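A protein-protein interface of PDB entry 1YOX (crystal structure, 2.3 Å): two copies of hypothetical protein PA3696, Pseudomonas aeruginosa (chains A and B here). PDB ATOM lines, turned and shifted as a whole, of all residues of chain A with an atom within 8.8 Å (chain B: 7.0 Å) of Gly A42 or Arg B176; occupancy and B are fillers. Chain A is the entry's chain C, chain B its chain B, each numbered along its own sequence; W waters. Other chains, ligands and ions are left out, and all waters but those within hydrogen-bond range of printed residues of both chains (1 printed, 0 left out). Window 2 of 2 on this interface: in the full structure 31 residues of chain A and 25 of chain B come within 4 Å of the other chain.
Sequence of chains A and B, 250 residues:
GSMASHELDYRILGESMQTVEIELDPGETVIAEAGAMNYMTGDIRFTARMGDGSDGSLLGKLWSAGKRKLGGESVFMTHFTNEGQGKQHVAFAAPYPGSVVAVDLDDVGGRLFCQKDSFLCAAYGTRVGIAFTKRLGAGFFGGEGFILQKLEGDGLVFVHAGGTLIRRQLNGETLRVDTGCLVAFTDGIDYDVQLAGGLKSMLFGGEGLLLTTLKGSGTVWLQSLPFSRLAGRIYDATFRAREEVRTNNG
Among the printed residues, pairs that only touch across the chains: Tyr A39 with Arg B176, Met A37 with Asp B178, Asn A38 with Val B177, Met A40 with Leu B175, Tyr A39 with Leu B222, Phe A46 with Arg B176 and Tyr A39 with Val B177.
O of Arg B176 sits at hydrogen-bond distance from N of Met A40 (2.9 Å).
The guanidinium group (NH2) of Arg B176 lies within hydrogen-bond range of the backbone carbonyl oxygen (O) of Thr A41 (2.9 Å).
The backbone carbonyl oxygen (O) of Gly A42 is in hydrogen-bond range of the guanidinium group (NH2) of Arg B176 (3.4 Å).
O of Ile A44 is in hydrogen-bond range of NH2 of Arg B176 (2.6 Å).
The backbone carbonyl oxygen (O) of Asn A38 lies within hydrogen-bond range of the backbone NH (N) of Asp B178, at 3.0 Å.
The guanidinium group (NH1) of Arg B176 sits close to the guanidinium group (NH1) of Arg A45 (3.1 Å).
Of chain B, only Arg B176 comes within 4 Å of Gly A42.
Printed residues of chain B within 4 Å of Ile A44: Arg B176.
Printed residues of chain B within 4 Å of Arg A45: Arg B176 (3.1 Å).
Printed residues of chain A within 4 Å of Leu B222: Tyr A39 (3.8 Å).
Printed residues of chain B within 4 Å of Met A37: Asp B178 (3.4 Å).
Thr B213 touches none of the printed residues of chain A.
Thr B212 touches none of the printed residues of chain A.
The nearest residue of chain A that does not touch Arg B176 is Asn A38 (4.3 Å).
The backbone NH of Leu B175 is in hydrogen-bond range of the backbone carbonyl oxygen of Leu B214.
SD of Met A37 is in hydrogen-bond range of N of Tyr A39.
The backbone carbonyl oxygen of Ala A91 sits at hydrogen-bond distance from the backbone NH of Asn A38 (2.8 Å).
The side-chain hydroxyl of Thr A41 lies within hydrogen-bond range of the side-chain amide oxygen of Gln A88.
The backbone NH (N) of His A89 is in hydrogen-bond range of the side-chain hydroxyl (OG1) of Thr A41 (2.8 Å).
The backbone NH (N) of Gly A42 is in hydrogen-bond range of the side-chain amide oxygen (OE1) of Gln A88 (3.3 Å).
Water W1 bridges the backbone carbonyl oxygen (O) of Met A37 and the side-chain carboxylate (OD2) of Asp B178.
No position is printed for both chains.
Of the 10 printed residues of chain B, 5 touch a printed residue of chain A.
Printed residues of chain B that touch a printed residue of chain A: Leu B175, Arg B176, Val B177, Asp B178 and Leu B222.
Hydrophobic or aromatic side chains of chain B that line the printed part of chain A: Leu B175, Val B177 and Leu B222.
Hydrophobic or aromatic side chains of chain A that line the printed part of chain B: Tyr A39, Met A40, Ile A44 and Phe A46.
Among the printed residues, 13 pairs touch across the chains.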
ATOM      1  N   MET A  37     -33.922   2.720  13.431  1.00  0.00           N
ATOM      2  CA  MET A  37     -32.630   2.968  12.800  1.00  0.00           C
ATOM      3  C   MET A  37     -32.431   2.177  11.498  1.00  0.00           C
ATOM      4  O   MET A  37     -32.674   0.956  11.451  1.00  0.00           O
ATOM      5  CB  MET A  37     -31.481   2.696  13.778  1.00  0.00           C
ATOM      6  CG  MET A  37     -30.852   1.327  13.623  1.00  0.00           C
ATOM      7  SD  MET A  37     -29.326   1.315  12.373  1.00  0.00           S
ATOM      8  CE  MET A  37     -28.597   2.793  13.275  1.00  0.00           C
ATOM      9  N   ASN A  38     -31.980   2.872  10.459  1.00  0.00           N
ATOM     10  CA  ASN A  38     -31.644   2.252   9.166  1.00  0.00           C
ATOM     11  C   ASN A  38     -30.155   1.954   9.015  1.00  0.00           C
ATOM     12  O   ASN A  38     -29.785   0.909   8.451  1.00  0.00           O
ATOM     13  CB  ASN A  38     -31.985   3.160   8.002  1.00  0.00           C
ATOM     14  CG  ASN A  38     -33.451   3.517   7.910  1.00  0.00           C
ATOM     15  OD1 ASN A  38     -33.770   4.621   7.476  1.00  0.00           O
ATOM     16  ND2 ASN A  38     -34.344   2.596   8.260  1.00  0.00           N
ATOM     17  N   TYR A  39     -29.312   2.904   9.434  1.00  0.00           N
ATOM     18  CA  TYR A  39     -27.872   2.771   9.320  1.00  0.00           C
ATOM     19  C   TYR A  39     -27.121   3.715  10.241  1.00  0.00           C
ATOM     20  O   TYR A  39     -27.631   4.747  10.664  1.00  0.00           O
ATOM     21  CB  TYR A  39     -27.372   2.920   7.860  1.00  0.00           C
ATOM     22  CG  TYR A  39     -27.538   4.312   7.270  1.00  0.00           C
ATOM     23  CD1 TYR A  39     -28.595   4.585   6.410  1.00  0.00           C
ATOM     24  CD2 TYR A  39     -26.649   5.353   7.577  1.00  0.00           C
ATOM     25  CE1 TYR A  39     -28.784   5.835   5.871  1.00  0.00           C
ATOM     26  CE2 TYR A  39     -26.846   6.644   7.034  1.00  0.00           C
ATOM     27  CZ  TYR A  39     -27.917   6.864   6.175  1.00  0.00           C
ATOM     28  OH  TYR A  39     -28.169   8.099   5.599  1.00  0.00           O
ATOM     29  N   MET A  40     -25.883   3.345  10.528  1.00  0.00           N
ATOM     30  CA  MET A  40     -25.004   4.165  11.333  1.00  0.00           C
ATOM     31  C   MET A  40     -23.560   3.962  10.908  1.00  0.00           C
ATOM     32  O   MET A  40     -23.139   2.846  10.581  1.00  0.00           O
ATOM     33  CB  MET A  40     -25.205   3.921  12.846  1.00  0.00           C
ATOM     34  CG  MET A  40     -25.145   2.493  13.283  1.00  0.00           C
ATOM     35  SD  MET A  40     -25.729   2.169  15.153  1.00  0.00           S
ATOM     36  CE  MET A  40     -25.703   0.172  14.929  1.00  0.00           C
ATOM     37  N   THR A  41     -22.830   5.070  10.892  1.00  0.00           N
ATOM     38  CA  THR A  41     -21.391   5.084  10.644  1.00  0.00           C
ATOM     39  C   THR A  41     -20.589   4.548  11.834  1.00  0.00           C
ATOM     40  O   THR A  41     -21.145   4.195  12.885  1.00  0.00           O
ATOM     41  CB  THR A  41     -20.887   6.512  10.209  1.00  0.00           C
ATOM     42  OG1 THR A  41     -21.237   7.465  11.210  1.00  0.00           O
ATOM     43  CG2 THR A  41     -21.489   6.943   8.887  1.00  0.00           C
ATOM     44  N   GLY A  42     -19.269   4.509  11.660  1.00  0.00           N
ATOM     45  CA  GLY A  42     -18.402   3.581  12.388  1.00  0.00           C
ATOM     46  C   GLY A  42     -18.243   3.795  13.871  1.00  0.00           C
ATOM     47  O   GLY A  42     -18.184   2.830  14.638  1.00  0.00           O
ATOM     48  N   ASP A  43     -18.167   5.046  14.294  1.00  0.00           N
ATOM     49  CA  ASP A  43     -17.936   5.330  15.714  1.00  0.00           C
ATOM     50  C   ASP A  43     -19.204   5.735  16.449  1.00  0.00           C
ATOM     51  O   ASP A  43     -19.118   6.337  17.516  1.00  0.00           O
ATOM     52  CB  ASP A  43     -16.839   6.410  15.895  1.00  0.00           C
ATOM     53  CG  ASP A  43     -15.644   6.223  14.944  1.00  0.00           C
ATOM     54  OD1 ASP A  43     -15.005   7.244  14.589  1.00  0.00           O
ATOM     55  OD2 ASP A  43     -15.354   5.065  14.543  1.00  0.00           O
ATOM     56  N   ILE A  44     -20.372   5.442  15.860  1.00  0.00           N
ATOM     57  CA  ILE A  44     -21.664   5.500  16.588  1.00  0.00           C
ATOM     58  C   ILE A  44     -21.837   4.316  17.541  1.00  0.00           C
ATOM     59  O   ILE A  44     -21.747   3.182  17.131  1.00  0.00           O
ATOM     60  CB  ILE A  44     -22.898   5.593  15.646  1.00  0.00           C
ATOM     61  CG1 ILE A  44     -23.062   7.021  15.144  1.00  0.00           C
ATOM     62  CG2 ILE A  44     -24.219   5.212  16.384  1.00  0.00           C
ATOM     63  CD1 ILE A  44     -22.645   7.156  13.754  1.00  0.00           C
ATOM     64  N   ARG A  45     -22.048   4.613  18.815  1.00  0.00           N
ATOM     65  CA  ARG A  45     -22.422   3.619  19.825  1.00  0.00           C
ATOM     66  C   ARG A  45     -23.865   3.851  20.306  1.00  0.00           C
ATOM     67  O   ARG A  45     -24.360   4.992  20.362  1.00  0.00           O
ATOM     68  CB  ARG A  45     -21.473   3.680  21.032  1.00  0.00           C
ATOM     69  CG  ARG A  45     -19.989   3.334  20.747  1.00  0.00           C
ATOM     70  CD  ARG A  45     -19.776   1.854  20.437  1.00  0.00           C
ATOM     71  NE  ARG A  45     -18.551   1.647  19.670  1.00  0.00           N
ATOM     72  CZ  ARG A  45     -18.494   1.533  18.344  1.00  0.00           C
ATOM     73  NH1 ARG A  45     -19.598   1.603  17.602  1.00  0.00           N
ATOM     74  NH2 ARG A  45     -17.320   1.363  17.757  1.00  0.00           N
ATOM     75  N   PHE A  46     -24.527   2.760  20.661  1.00  0.00           N
ATOM     76  CA  PHE A  46     -25.941   2.794  21.064  1.00  0.00           C
ATOM     77  C   PHE A  46     -26.150   2.112  22.416  1.00  0.00           C
ATOM     78  O   PHE A  46     -25.565   1.055  22.686  1.00  0.00           O
ATOM     79  CB  PHE A  46     -26.802   2.122  19.999  1.00  0.00           C
ATOM     80  CG  PHE A  46     -26.289   0.778  19.572  1.00  0.00           C
ATOM     81  CD1 PHE A  46     -26.552  -0.360  20.334  1.00  0.00           C
ATOM     82  CD2 PHE A  46     -25.534   0.650  18.418  1.00  0.00           C
ATOM     83  CE1 PHE A  46     -26.072  -1.613  19.947  1.00  0.00           C
ATOM     84  CE2 PHE A  46     -25.049  -0.596  18.013  1.00  0.00           C
ATOM     85  CZ  PHE A  46     -25.317  -1.732  18.778  1.00  0.00           C
ATOM     86  N   PHE A  80     -28.152   7.026  20.808  1.00  0.00           N
ATOM     87  CA  PHE A  80     -27.059   6.884  19.835  1.00  0.00           C
ATOM     88  C   PHE A  80     -26.051   8.018  20.050  1.00  0.00           C
ATOM     89  O   PHE A  80     -26.380   9.182  19.888  1.00  0.00           O
ATOM     90  CB  PHE A  80     -27.611   6.881  18.398  1.00  0.00           C
ATOM     91  CG  PHE A  80     -28.511   5.706  18.103  1.00  0.00           C
ATOM     92  CD1 PHE A  80     -29.849   5.702  18.528  1.00  0.00           C
ATOM     93  CD2 PHE A  80     -28.025   4.592  17.435  1.00  0.00           C
ATOM     94  CE1 PHE A  80     -30.679   4.603  18.279  1.00  0.00           C
ATOM     95  CE2 PHE A  80     -28.870   3.487  17.161  1.00  0.00           C
ATOM     96  CZ  PHE A  80     -30.188   3.500  17.580  1.00  0.00           C
ATOM     97  N   THR A  81     -24.830   7.667  20.438  1.00  0.00           N
ATOM     98  CA  THR A  81     -23.785   8.666  20.670  1.00  0.00           C
ATOM     99  C   THR A  81     -22.609   8.520  19.714  1.00  0.00           C
ATOM    100  O   THR A  81     -22.209   7.392  19.351  1.00  0.00           O
ATOM    101  CB  THR A  81     -23.305   8.664  22.138  1.00  0.00           C
ATOM    102  OG1 THR A  81     -24.448   8.753  22.983  1.00  0.00           O
ATOM    103  CG2 THR A  81     -22.414   9.884  22.438  1.00  0.00           C
ATOM    104  N   ASN A  82     -22.083   9.680  19.298  1.00  0.00           N
ATOM    105  CA  ASN A  82     -20.803   9.773  18.580  1.00  0.00           C
ATOM    106  C   ASN A  82     -19.592   9.649  19.541  1.00  0.00           C
ATOM    107  O   ASN A  82     -19.280  10.579  20.304  1.00  0.00           O
ATOM    108  CB  ASN A  82     -20.749  11.082  17.812  1.00  0.00           C
ATOM    109  CG  ASN A  82     -19.493  11.231  16.940  1.00  0.00           C
ATOM    110  OD1 ASN A  82     -19.401  12.165  16.136  1.00  0.00           O
ATOM    111  ND2 ASN A  82     -18.553  10.322  17.077  1.00  0.00           N
ATOM    112  N   GLU A  83     -18.936   8.491  19.486  1.00  0.00           N
ATOM    113  CA  GLU A  83     -17.787   8.178  20.334  1.00  0.00           C
ATOM    114  C   GLU A  83     -16.462   8.358  19.597  1.00  0.00           C
ATOM    115  O   GLU A  83     -15.413   7.885  20.067  1.00  0.00           O
ATOM    116  CB  GLU A  83     -17.860   6.722  20.808  1.00  0.00           C
ATOM    117  CG  GLU A  83     -19.181   6.331  21.416  1.00  0.00           C
ATOM    118  CD  GLU A  83     -19.146   6.379  22.921  1.00  0.00           C
ATOM    119  OE1 GLU A  83     -18.793   5.334  23.512  1.00  0.00           O
ATOM    120  OE2 GLU A  83     -19.436   7.454  23.506  1.00  0.00           O
ATOM    121  N   GLY A  84     -16.513   8.998  18.433  1.00  0.00           N
ATOM    122  CA  GLY A  84     -15.316   9.247  17.632  1.00  0.00           C
ATOM    123  C   GLY A  84     -14.811  10.663  17.781  1.00  0.00           C
ATOM    124  O   GLY A  84     -15.073  11.323  18.799  1.00  0.00           O
ATOM    125  N   LYS A  87     -17.276  14.068  12.638  1.00  0.00           N
ATOM    126  CA  LYS A  87     -18.704  13.916  12.354  1.00  0.00           C
ATOM    127  C   LYS A  87     -19.112  12.470  12.062  1.00  0.00           C
ATOM    128  O   LYS A  87     -18.483  11.799  11.218  1.00  0.00           O
ATOM    129  CB  LYS A  87     -19.097  14.749  11.128  1.00  0.00           C
ATOM    130  CG  LYS A  87     -19.481  16.169  11.422  1.00  0.00           C
ATOM    131  CD  LYS A  87     -19.731  16.936  10.112  1.00  0.00           C
ATOM    132  CE  LYS A  87     -19.754  18.447  10.373  1.00  0.00           C
ATOM    133  NZ  LYS A  87     -19.996  19.230   9.128  1.00  0.00           N
ATOM    134  N   GLN A  88     -20.186  12.023  12.718  1.00  0.00           N
ATOM    135  CA  GLN A  88     -20.765  10.726  12.424  1.00  0.00           C
ATOM    136  C   GLN A  88     -22.260  10.849  12.118  1.00  0.00           C
ATOM    137  O   GLN A  88     -22.893  11.885  12.367  1.00  0.00           O
ATOM    138  CB  GLN A  88     -20.543   9.759  13.582  1.00  0.00           C
ATOM    139  CG  GLN A  88     -19.094   9.488  13.967  1.00  0.00           C
ATOM    140  CD  GLN A  88     -18.340   8.678  12.937  1.00  0.00           C
ATOM    141  OE1 GLN A  88     -18.883   7.759  12.340  1.00  0.00           O
ATOM    142  NE2 GLN A  88     -17.066   9.022  12.722  1.00  0.00           N
ATOM    143  N   HIS A  89     -22.833   9.778  11.586  1.00  0.00           N
ATOM    144  CA  HIS A  89     -24.201   9.823  11.116  1.00  0.00           C
ATOM    145  C   HIS A  89     -24.980   8.578  11.526  1.00  0.00           C
ATOM    146  O   HIS A  89     -24.412   7.466  11.596  1.00  0.00           O
ATOM    147  CB  HIS A  89     -24.227   9.990   9.601  1.00  0.00           C
ATOM    148  CG  HIS A  89     -23.469  11.184   9.114  1.00  0.00           C
ATOM    149  ND1 HIS A  89     -24.069  12.401   8.854  1.00  0.00           N
ATOM    150  CD2 HIS A  89     -22.154  11.341   8.815  1.00  0.00           C
ATOM    151  CE1 HIS A  89     -23.152  13.257   8.432  1.00  0.00           C
ATOM    152  NE2 HIS A  89     -21.985  12.638   8.403  1.00  0.00           N
ATOM    153  N   VAL A  90     -26.274   8.784  11.798  1.00  0.00           N
ATOM    154  CA  VAL A  90     -27.248   7.708  12.020  1.00  0.00           C
ATOM    155  C   VAL A  90     -28.566   8.132  11.374  1.00  0.00           C
ATOM    156  O   VAL A  90     -29.020   9.234  11.625  1.00  0.00           O
ATOM    157  CB  VAL A  90     -27.595   7.506  13.518  1.00  0.00           C
ATOM    158  CG1 VAL A  90     -28.212   6.134  13.749  1.00  0.00           C
ATOM    159  CG2 VAL A  90     -26.418   7.727  14.421  1.00  0.00           C
ATOM    160  N   ALA A  91     -29.193   7.251  10.596  1.00  0.00           N
ATOM    161  CA  ALA A  91     -30.489   7.538   9.982  1.00  0.00           C
ATOM    162  C   ALA A  91     -31.669   6.741  10.617  1.00  0.00           C
ATOM    163  O   ALA A  91     -31.487   5.601  11.092  1.00  0.00           O
ATOM    164  CB  ALA A  91     -30.430   7.328   8.458  1.00  0.00           C
ATOM    165  N   THR B 174     -16.484   0.966   7.371  1.00  0.00           N
ATOM    166  CA  THR B 174     -17.466   0.031   7.895  1.00  0.00           C
ATOM    167  C   THR B 174     -18.783   0.788   8.075  1.00  0.00           C
ATOM    168  O   THR B 174     -18.800   1.901   8.575  1.00  0.00           O
ATOM    169  CB  THR B 174     -17.022  -0.537   9.258  1.00  0.00           C
ATOM    170  OG1 THR B 174     -16.660   0.552  10.114  1.00  0.00           O
ATOM    171  CG2 THR B 174     -15.822  -1.428   9.123  1.00  0.00           C
ATOM    172  N   LEU B 175     -19.874   0.171   7.659  1.00  0.00           N
ATOM    173  CA  LEU B 175     -21.217   0.715   7.829  1.00  0.00           C
ATOM    174  C   LEU B 175     -22.107  -0.343   8.520  1.00  0.00           C
ATOM    175  O   LEU B 175     -22.102  -1.521   8.151  1.00  0.00           O
ATOM    176  CB  LEU B 175     -21.797   1.087   6.439  1.00  0.00           C
ATOM    177  CG  LEU B 175     -23.180   1.761   6.300  1.00  0.00           C
ATOM    178  CD1 LEU B 175     -23.223   3.141   6.990  1.00  0.00           C
ATOM    179  CD2 LEU B 175     -23.632   1.874   4.837  1.00  0.00           C
ATOM    180  N   ARG B 176     -22.893   0.076   9.495  1.00  0.00           N
ATOM    181  CA  ARG B 176     -23.801  -0.866  10.149  1.00  0.00           C
ATOM    182  C   ARG B 176     -25.247  -0.577   9.756  1.00  0.00           C
ATOM    183  O   ARG B 176     -25.720   0.544   9.882  1.00  0.00           O
ATOM    184  CB  ARG B 176     -23.588  -0.872  11.665  1.00  0.00           C
ATOM    185  CG  ARG B 176     -22.359  -1.692  12.119  1.00  0.00           C
ATOM    186  CD  ARG B 176     -21.976  -1.368  13.574  1.00  0.00           C
ATOM    187  NE  ARG B 176     -21.771   0.078  13.717  1.00  0.00           N
ATOM    188  CZ  ARG B 176     -21.704   0.747  14.863  1.00  0.00           C
ATOM    189  NH1 ARG B 176     -21.818   0.106  16.030  1.00  0.00           N
ATOM    190  NH2 ARG B 176     -21.505   2.064  14.837  1.00  0.00           N
ATOM    191  N   VAL B 177     -25.939  -1.593   9.242  1.00  0.00           N
ATOM    192  CA  VAL B 177     -27.292  -1.384   8.752  1.00  0.00           C
ATOM    193  C   VAL B 177     -28.290  -2.355   9.379  1.00  0.00           C
ATOM    194  O   VAL B 177     -27.943  -3.495   9.682  1.00  0.00           O
ATOM    195  CB  VAL B 177     -27.380  -1.387   7.179  1.00  0.00           C
ATOM    196  CG1 VAL B 177     -26.173  -0.641   6.557  1.00  0.00           C
ATOM    197  CG2 VAL B 177     -27.499  -2.785   6.596  1.00  0.00           C
ATOM    198  N   ASP B 178     -29.516  -1.884   9.585  1.00  0.00           N
ATOM    199  CA  ASP B 178     -30.646  -2.765   9.795  1.00  0.00           C
ATOM    200  C   ASP B 178     -30.701  -3.736   8.614  1.00  0.00           C
ATOM    201  O   ASP B 178     -30.672  -3.333   7.451  1.00  0.00           O
ATOM    202  CB  ASP B 178     -31.919  -1.940   9.875  1.00  0.00           C
ATOM    203  CG  ASP B 178     -33.129  -2.765  10.313  1.00  0.00           C
ATOM    204  OD1 ASP B 178     -33.745  -3.382   9.455  1.00  0.00           O
ATOM    205  OD2 ASP B 178     -33.492  -2.756  11.513  1.00  0.00           O
ATOM    206  N   LEU B 211     -28.613  -7.037  12.689  1.00  0.00           N
ATOM    207  CA  LEU B 211     -27.674  -6.001  12.231  1.00  0.00           C
ATOM    208  C   LEU B 211     -26.714  -6.592  11.206  1.00  0.00           C
ATOM    209  O   LEU B 211     -26.039  -7.613  11.462  1.00  0.00           O
ATOM    210  CB  LEU B 211     -26.851  -5.446  13.391  1.00  0.00           C
ATOM    211  CG  LEU B 211     -26.638  -3.965  13.726  1.00  0.00           C
ATOM    212  CD1 LEU B 211     -25.175  -3.743  14.043  1.00  0.00           C
ATOM    213  CD2 LEU B 211     -27.119  -2.958  12.678  1.00  0.00           C
ATOM    214  N   THR B 212     -26.651  -5.937  10.052  1.00  0.00           N
ATOM    215  CA  THR B 212     -25.639  -6.255   9.058  1.00  0.00           C
ATOM    216  C   THR B 212     -24.447  -5.303   9.133  1.00  0.00           C
ATOM    217  O   THR B 212     -24.618  -4.086   9.057  1.00  0.00           O
ATOM    218  CB  THR B 212     -26.250  -6.248   7.666  1.00  0.00           C
ATOM    219  OG1 THR B 212     -27.208  -7.312   7.592  1.00  0.00           O
ATOM    220  CG2 THR B 212     -25.171  -6.436   6.585  1.00  0.00           C
ATOM    221  N   THR B 213     -23.246  -5.862   9.284  1.00  0.00           N
ATOM    222  CA  THR B 213     -22.014  -5.066   9.252  1.00  0.00           C
ATOM    223  C   THR B 213     -21.403  -5.185   7.852  1.00  0.00           C
ATOM    224  O   THR B 213     -21.216  -6.295   7.334  1.00  0.00           O
ATOM    225  CB  THR B 213     -21.035  -5.482  10.357  1.00  0.00           C
ATOM    226  OG1 THR B 213     -21.704  -5.400  11.624  1.00  0.00           O
ATOM    227  CG2 THR B 213     -19.806  -4.532  10.412  1.00  0.00           C
ATOM    228  N   LEU B 214     -21.194  -4.049   7.201  1.00  0.00           N
ATOM    229  CA  LEU B 214     -20.644  -4.013   5.839  1.00  0.00           C
ATOM    230  C   LEU B 214     -19.287  -3.326   5.859  1.00  0.00           C
ATOM    231  O   LEU B 214     -19.138  -2.279   6.506  1.00  0.00           O
ATOM    232  CB  LEU B 214     -21.554  -3.234   4.889  1.00  0.00           C
ATOM    233  CG  LEU B 214     -22.958  -3.767   4.622  1.00  0.00           C
ATOM    234  CD1 LEU B 214     -23.765  -2.603   4.052  1.00  0.00           C
ATOM    235  CD2 LEU B 214     -22.952  -4.964   3.672  1.00  0.00           C
ATOM    236  N   LEU B 222     -29.368   1.030  -0.088  1.00  0.00           N
ATOM    237  CA  LEU B 222     -30.191   0.886   1.096  1.00  0.00           C
ATOM    238  C   LEU B 222     -31.605   1.381   0.821  1.00  0.00           C
ATOM    239  O   LEU B 222     -31.818   2.238  -0.044  1.00  0.00           O
ATOM    240  CB  LEU B 222     -29.585   1.682   2.266  1.00  0.00           C
ATOM    241  CG  LEU B 222     -28.137   1.344   2.697  1.00  0.00           C
ATOM    242  CD1 LEU B 222     -27.443   2.432   3.547  1.00  0.00           C
ATOM    243  CD2 LEU B 222     -28.038   0.002   3.370  1.00  0.00           C
HETATM  244  O   HOH W   1     -32.852  -0.639  13.471  1.00  0.00           O
